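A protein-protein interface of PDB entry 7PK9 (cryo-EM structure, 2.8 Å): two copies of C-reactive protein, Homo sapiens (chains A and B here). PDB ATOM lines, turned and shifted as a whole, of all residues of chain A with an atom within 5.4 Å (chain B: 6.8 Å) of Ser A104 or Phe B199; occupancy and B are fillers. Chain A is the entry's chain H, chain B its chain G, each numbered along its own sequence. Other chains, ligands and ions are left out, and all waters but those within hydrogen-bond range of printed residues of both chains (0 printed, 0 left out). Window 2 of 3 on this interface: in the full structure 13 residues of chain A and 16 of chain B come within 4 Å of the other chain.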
ATOM      1  N   GLU A 101      -7.929  15.254   5.342  1.00  0.00           N
ATOM      2  CA  GLU A 101      -7.064  14.129   5.001  1.00  0.00           C
ATOM      3  C   GLU A 101      -6.380  13.594   6.254  1.00  0.00           C
ATOM      4  O   GLU A 101      -5.619  14.312   6.908  1.00  0.00           O
ATOM      5  CB  GLU A 101      -6.037  14.564   3.956  1.00  0.00           C
ATOM      6  CG  GLU A 101      -4.920  13.598   3.705  1.00  0.00           C
ATOM      7  CD  GLU A 101      -3.941  14.114   2.675  1.00  0.00           C
ATOM      8  OE1 GLU A 101      -2.895  14.675   3.057  1.00  0.00           O
ATOM      9  OE2 GLU A 101      -4.225  13.966   1.475  1.00  0.00           O
ATOM     10  N   SER A 102      -6.627  12.322   6.561  1.00  0.00           N
ATOM     11  CA  SER A 102      -5.908  11.630   7.628  1.00  0.00           C
ATOM     12  C   SER A 102      -4.393  11.724   7.482  1.00  0.00           C
ATOM     13  O   SER A 102      -3.686  12.038   8.444  1.00  0.00           O
ATOM     14  CB  SER A 102      -6.336  10.169   7.676  1.00  0.00           C
ATOM     15  OG  SER A 102      -5.564   9.464   8.624  1.00  0.00           O
ATOM     16  N   ALA A 103      -3.871  11.442   6.289  1.00  0.00           N
ATOM     17  CA  ALA A 103      -2.426  11.335   6.107  1.00  0.00           C
ATOM     18  C   ALA A 103      -1.676  12.533   6.663  1.00  0.00           C
ATOM     19  O   ALA A 103      -0.521  12.402   7.079  1.00  0.00           O
ATOM     20  CB  ALA A 103      -2.096  11.172   4.625  1.00  0.00           C
ATOM     21  N   SER A 104      -2.302  13.700   6.678  1.00  0.00           N
ATOM     22  CA  SER A 104      -1.696  14.909   7.206  1.00  0.00           C
ATOM     23  C   SER A 104      -2.582  15.626   8.213  1.00  0.00           C
ATOM     24  O   SER A 104      -2.090  16.513   8.914  1.00  0.00           O
ATOM     25  CB  SER A 104      -1.350  15.865   6.059  1.00  0.00           C
ATOM     26  OG  SER A 104      -2.512  16.204   5.334  1.00  0.00           O
ATOM     27  N   GLY A 105      -3.854  15.263   8.316  1.00  0.00           N
ATOM     28  CA  GLY A 105      -4.851  16.021   9.040  1.00  0.00           C
ATOM     29  C   GLY A 105      -5.195  17.397   8.520  1.00  0.00           C
ATOM     30  O   GLY A 105      -5.959  18.113   9.166  1.00  0.00           O
ATOM     31  N   ILE A 106      -4.636  17.808   7.384  1.00  0.00           N
ATOM     32  CA  ILE A 106      -4.983  19.113   6.839  1.00  0.00           C
ATOM     33  C   ILE A 106      -6.489  19.169   6.612  1.00  0.00           C
ATOM     34  O   ILE A 106      -7.057  18.349   5.885  1.00  0.00           O
ATOM     35  CB  ILE A 106      -4.177  19.392   5.580  1.00  0.00           C
ATOM     36  CG1 ILE A 106      -2.746  19.716   5.999  1.00  0.00           C
ATOM     37  CG2 ILE A 106      -4.764  20.553   4.814  1.00  0.00           C
ATOM     38  CD1 ILE A 106      -1.788  19.826   4.878  1.00  0.00           C
ATOM     39  N   SER A 120      -4.431  21.849  10.545  1.00  0.00           N
ATOM     40  CA  SER A 120      -4.345  20.416  10.826  1.00  0.00           C
ATOM     41  C   SER A 120      -5.307  19.987  11.929  1.00  0.00           C
ATOM     42  O   SER A 120      -5.427  20.651  12.959  1.00  0.00           O
ATOM     43  CB  SER A 120      -2.916  20.054  11.226  1.00  0.00           C
ATOM     44  OG  SER A 120      -2.733  18.657  11.282  1.00  0.00           O
ATOM     45  N   LEU A 121      -5.991  18.863  11.696  1.00  0.00           N
ATOM     46  CA  LEU A 121      -6.877  18.223  12.662  1.00  0.00           C
ATOM     47  C   LEU A 121      -6.801  16.706  12.578  1.00  0.00           C
ATOM     48  O   LEU A 121      -6.923  16.146  11.487  1.00  0.00           O
ATOM     49  CB  LEU A 121      -8.324  18.661  12.436  1.00  0.00           C
ATOM     50  CG  LEU A 121      -9.380  18.079  13.375  1.00  0.00           C
ATOM     51  CD1 LEU A 121      -9.129  18.486  14.810  1.00  0.00           C
ATOM     52  CD2 LEU A 121     -10.743  18.504  12.929  1.00  0.00           C
ATOM     53  N   LYS A 123      -4.676  14.252  12.663  1.00  0.00           N
ATOM     54  CA  LYS A 123      -3.728  13.508  11.844  1.00  0.00           C
ATOM     55  C   LYS A 123      -3.656  12.043  12.263  1.00  0.00           C
ATOM     56  O   LYS A 123      -3.619  11.727  13.453  1.00  0.00           O
ATOM     57  CB  LYS A 123      -2.349  14.155  11.917  1.00  0.00           C
ATOM     58  CG  LYS A 123      -1.325  13.501  11.013  1.00  0.00           C
ATOM     59  CD  LYS A 123       0.034  14.089  11.232  1.00  0.00           C
ATOM     60  CE  LYS A 123       1.106  13.304  10.514  1.00  0.00           C
ATOM     61  NZ  LYS A 123       2.466  13.678  10.992  1.00  0.00           N
ATOM     62  N   ALA B   8       2.189  24.611  -3.066  1.00  0.00           N
ATOM     63  CA  ALA B   8       2.572  25.427  -1.928  1.00  0.00           C
ATOM     64  C   ALA B   8       3.099  24.547  -0.811  1.00  0.00           C
ATOM     65  O   ALA B   8       2.711  23.387  -0.676  1.00  0.00           O
ATOM     66  CB  ALA B   8       1.391  26.254  -1.409  1.00  0.00           C
ATOM     67  N   PHE B   9       3.995  25.111  -0.016  1.00  0.00           N
ATOM     68  CA  PHE B   9       4.340  24.528   1.271  1.00  0.00           C
ATOM     69  C   PHE B   9       3.304  24.910   2.314  1.00  0.00           C
ATOM     70  O   PHE B   9       2.945  26.078   2.443  1.00  0.00           O
ATOM     71  CB  PHE B   9       5.721  24.994   1.711  1.00  0.00           C
ATOM     72  CG  PHE B   9       6.823  24.515   0.837  1.00  0.00           C
ATOM     73  CD1 PHE B   9       7.034  23.169   0.653  1.00  0.00           C
ATOM     74  CD2 PHE B   9       7.663  25.405   0.212  1.00  0.00           C
ATOM     75  CE1 PHE B   9       8.057  22.729  -0.139  1.00  0.00           C
ATOM     76  CE2 PHE B   9       8.684  24.961  -0.580  1.00  0.00           C
ATOM     77  CZ  PHE B   9       8.880  23.628  -0.757  1.00  0.00           C
ATOM     78  N   VAL B  10       2.822  23.921   3.054  1.00  0.00           N
ATOM     79  CA  VAL B  10       1.829  24.131   4.094  1.00  0.00           C
ATOM     80  C   VAL B  10       2.489  23.864   5.435  1.00  0.00           C
ATOM     81  O   VAL B  10       3.025  22.778   5.667  1.00  0.00           O
ATOM     82  CB  VAL B  10       0.609  23.227   3.889  1.00  0.00           C
ATOM     83  CG1 VAL B  10      -0.508  23.614   4.815  1.00  0.00           C
ATOM     84  CG2 VAL B  10       0.156  23.309   2.459  1.00  0.00           C
ATOM     85  N   PHE B  11       2.440  24.851   6.313  1.00  0.00           N
ATOM     86  CA  PHE B  11       2.904  24.736   7.684  1.00  0.00           C
ATOM     87  C   PHE B  11       1.683  24.744   8.589  1.00  0.00           C
ATOM     88  O   PHE B  11       1.320  25.800   9.116  1.00  0.00           O
ATOM     89  CB  PHE B  11       3.825  25.899   8.019  1.00  0.00           C
ATOM     90  CG  PHE B  11       5.077  25.918   7.213  1.00  0.00           C
ATOM     91  CD1 PHE B  11       6.214  25.284   7.654  1.00  0.00           C
ATOM     92  CD2 PHE B  11       5.114  26.581   6.004  1.00  0.00           C
ATOM     93  CE1 PHE B  11       7.353  25.307   6.898  1.00  0.00           C
ATOM     94  CE2 PHE B  11       6.245  26.607   5.252  1.00  0.00           C
ATOM     95  CZ  PHE B  11       7.362  25.967   5.688  1.00  0.00           C
ATOM     96  N   PRO B  12       1.003  23.615   8.783  1.00  0.00           N
ATOM     97  CA  PRO B  12      -0.362  23.678   9.309  1.00  0.00           C
ATOM     98  C   PRO B  12      -0.454  23.830  10.811  1.00  0.00           C
ATOM     99  O   PRO B  12      -1.525  24.205  11.303  1.00  0.00           O
ATOM    100  CB  PRO B  12      -0.953  22.339   8.865  1.00  0.00           C
ATOM    101  CG  PRO B  12       0.199  21.427   8.929  1.00  0.00           C
ATOM    102  CD  PRO B  12       1.380  22.237   8.443  1.00  0.00           C
ATOM    103  N   LYS B  13       0.628  23.617  11.550  1.00  0.00           N
ATOM    104  CA  LYS B  13       0.642  23.822  12.987  1.00  0.00           C
ATOM    105  C   LYS B  13       1.875  24.613  13.384  1.00  0.00           C
ATOM    106  O   LYS B  13       2.884  24.632  12.676  1.00  0.00           O
ATOM    107  CB  LYS B  13       0.605  22.496  13.742  1.00  0.00           C
ATOM    108  CG  LYS B  13       1.783  21.593  13.465  1.00  0.00           C
ATOM    109  CD  LYS B  13       1.477  20.166  13.891  1.00  0.00           C
ATOM    110  CE  LYS B  13       0.871  19.335  12.768  1.00  0.00           C
ATOM    111  NZ  LYS B  13       1.665  19.342  11.507  1.00  0.00           N
ATOM    112  N   VAL B  20      11.432  24.671   5.754  1.00  0.00           N
ATOM    113  CA  VAL B  20      12.084  24.265   4.513  1.00  0.00           C
ATOM    114  C   VAL B  20      13.241  25.204   4.210  1.00  0.00           C
ATOM    115  O   VAL B  20      13.109  26.426   4.320  1.00  0.00           O
ATOM    116  CB  VAL B  20      11.085  24.222   3.342  1.00  0.00           C
ATOM    117  CG1 VAL B  20       9.880  23.404   3.723  1.00  0.00           C
ATOM    118  CG2 VAL B  20      10.645  25.595   2.934  1.00  0.00           C
ATOM    119  N   ASP B 155       0.437  28.929   4.496  1.00  0.00           N
ATOM    120  CA  ASP B 155       0.971  28.521   3.206  1.00  0.00           C
ATOM    121  C   ASP B 155       1.916  29.570   2.665  1.00  0.00           C
ATOM    122  O   ASP B 155       1.674  30.768   2.809  1.00  0.00           O
ATOM    123  CB  ASP B 155      -0.138  28.319   2.181  1.00  0.00           C
ATOM    124  CG  ASP B 155      -1.094  27.226   2.564  1.00  0.00           C
ATOM    125  OD1 ASP B 155      -0.667  26.296   3.252  1.00  0.00           O
ATOM    126  OD2 ASP B 155      -2.270  27.282   2.163  1.00  0.00           O
ATOM    127  N   VAL B 194      13.043  19.666   3.207  1.00  0.00           N
ATOM    128  CA  VAL B 194      11.898  19.812   4.091  1.00  0.00           C
ATOM    129  C   VAL B 194      12.217  19.106   5.395  1.00  0.00           C
ATOM    130  O   VAL B 194      12.545  17.915   5.406  1.00  0.00           O
ATOM    131  CB  VAL B 194      10.627  19.234   3.462  1.00  0.00           C
ATOM    132  CG1 VAL B 194       9.480  19.364   4.416  1.00  0.00           C
ATOM    133  CG2 VAL B 194      10.315  19.946   2.170  1.00  0.00           C
ATOM    134  N   GLY B 196      10.685  18.384   9.318  1.00  0.00           N
ATOM    135  CA  GLY B 196       9.461  18.265  10.080  1.00  0.00           C
ATOM    136  C   GLY B 196       8.155  18.270   9.297  1.00  0.00           C
ATOM    137  O   GLY B 196       8.089  17.947   8.114  1.00  0.00           O
ATOM    138  N   GLU B 197       7.092  18.634  10.016  1.00  0.00           N
ATOM    139  CA  GLU B 197       5.717  18.627   9.508  1.00  0.00           C
ATOM    140  C   GLU B 197       5.464  19.763   8.523  1.00  0.00           C
ATOM    141  O   GLU B 197       4.879  20.796   8.849  1.00  0.00           O
ATOM    142  CB  GLU B 197       4.709  18.697  10.648  1.00  0.00           C
ATOM    143  CG  GLU B 197       4.643  17.480  11.566  1.00  0.00           C
ATOM    144  CD  GLU B 197       5.698  17.492  12.655  1.00  0.00           C
ATOM    145  OE1 GLU B 197       6.457  18.481  12.744  1.00  0.00           O
ATOM    146  OE2 GLU B 197       5.751  16.522  13.445  1.00  0.00           O
ATOM    147  N   VAL B 198       5.894  19.549   7.284  1.00  0.00           N
ATOM    148  CA  VAL B 198       5.607  20.452   6.178  1.00  0.00           C
ATOM    149  C   VAL B 198       5.116  19.611   5.017  1.00  0.00           C
ATOM    150  O   VAL B 198       5.664  18.543   4.729  1.00  0.00           O
ATOM    151  CB  VAL B 198       6.845  21.265   5.764  1.00  0.00           C
ATOM    152  CG1 VAL B 198       6.468  22.330   4.775  1.00  0.00           C
ATOM    153  CG2 VAL B 198       7.487  21.873   6.973  1.00  0.00           C
ATOM    154  N   PHE B 199       4.088  20.103   4.346  1.00  0.00           N
ATOM    155  CA  PHE B 199       3.460  19.416   3.235  1.00  0.00           C
ATOM    156  C   PHE B 199       3.540  20.248   1.965  1.00  0.00           C
ATOM    157  O   PHE B 199       3.522  21.478   2.012  1.00  0.00           O
ATOM    158  CB  PHE B 199       2.025  19.120   3.604  1.00  0.00           C
ATOM    159  CG  PHE B 199       1.910  18.335   4.866  1.00  0.00           C
ATOM    160  CD1 PHE B 199       1.674  18.979   6.060  1.00  0.00           C
ATOM    161  CD2 PHE B 199       2.107  16.973   4.877  1.00  0.00           C
ATOM    162  CE1 PHE B 199       1.598  18.275   7.230  1.00  0.00           C
ATOM    163  CE2 PHE B 199       2.023  16.266   6.045  1.00  0.00           C
ATOM    164  CZ  PHE B 199       1.775  16.916   7.224  1.00  0.00           C
ATOM    165  N   THR B 200       3.647  19.573   0.832  1.00  0.00           N
ATOM    166  CA  THR B 200       3.439  20.198  -0.462  1.00  0.00           C
ATOM    167  C   THR B 200       2.003  19.936  -0.884  1.00  0.00           C
ATOM    168  O   THR B 200       1.554  18.788  -0.874  1.00  0.00           O
ATOM    169  CB  THR B 200       4.407  19.653  -1.508  1.00  0.00           C
ATOM    170  OG1 THR B 200       5.750  19.879  -1.081  1.00  0.00           O
ATOM    171  CG2 THR B 200       4.204  20.358  -2.816  1.00  0.00           C
ATOM    172  N   LYS B 201       1.278  20.993  -1.218  1.00  0.00           N
ATOM    173  CA  LYS B 201      -0.128  20.900  -1.574  1.00  0.00           C
ATOM    174  C   LYS B 201      -0.406  21.820  -2.747  1.00  0.00           C
ATOM    175  O   LYS B 201       0.384  22.723  -3.033  1.00  0.00           O
ATOM    176  CB  LYS B 201      -1.027  21.298  -0.397  1.00  0.00           C
ATOM    177  CG  LYS B 201      -1.040  20.337   0.759  1.00  0.00           C
ATOM    178  CD  LYS B 201      -1.570  18.984   0.364  1.00  0.00           C
ATOM    179  CE  LYS B 201      -1.637  18.075   1.556  1.00  0.00           C
ATOM    180  NZ  LYS B 201      -2.739  17.096   1.452  1.00  0.00           N
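The side-chain amino group of Lys B201 is in salt-bridge range of the side-chain carboxylate of Glu A101 (2.9 Å).
The side-chain hydroxyl (OG) of Ser A104 sits close to the backbone NH (N) of Ile A106, 3.4 Å away.
OE1 of Glu A101 is in hydrogen-bond range of OG of Ser A104, at 2.8 Å.
O of Ser A104 sits at hydrogen-bond distance from OG of Ser A120, at 3.3 Å.
The backbone NH of Ala B8 lies within hydrogen-bond range of the backbone carbonyl oxygen of Lys B201, at 2.6 Å.
The backbone NH (N) of Glu A101 lies within hydrogen-bond range of the backbone carbonyl oxygen (O) of Ile A106 (3.3 Å).
The backbone NH of Val B10 is in hydrogen-bond range of the backbone carbonyl oxygen of Phe B199 (2.7 Å).
Phe B199 touches Ser A104 (CE2 to CB, 3.4 Å).
Lys B201 touches Ser A104.
Ile A106 touches Val B10 (CD1 to CG1, 3.999 Å).
Ile A106 touches Phe B199.
Lys B201 touches Ile A106.
Ser A120 touches Pro B12.
Ser A120 touches Lys B13.
Of the printed residues of chain B, Ser A104 touches Phe B199 (3.4 Å) and Lys B201 (3.99 Å).
Phe B199 touches two residues of chain A.
Printed residues of chain B within 4 Å of Ile A106: Val B10, Phe B199 and Lys B201.
Printed residues of chain A within 4 Å of Val B10: Ile A106 (3.999 Å).
Val B198 touches none of the printed residues of chain A.
The nearest printed residue of chain B that does not touch Ser A104 is Lys B13 (5.4 Å).
Of the 15 printed residues of chain B, 5 touch a printed residue of chain A.
Printed residues of chain B that touch a printed residue of chain A: Val B10, Pro B12, Lys B13, Phe B199 and Lys B201.
Hydrophobic or aromatic side chains of chain B within 4 Å of the printed part of chain A: Val B10, Pro B12 and Phe B199.
Of the 9 printed residues of chain A, 4 touch a printed residue of chain B.
Hydrophobic or aromatic side chains of chain A that line the printed part of chain B: Ile A106.
Among the printed residues, Asp or Glu carboxylates within 4 Å of a Lys or Arg side-chain nitrogen of the other chain: Glu A101 with Lys B201.
No position is printed for both chains.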
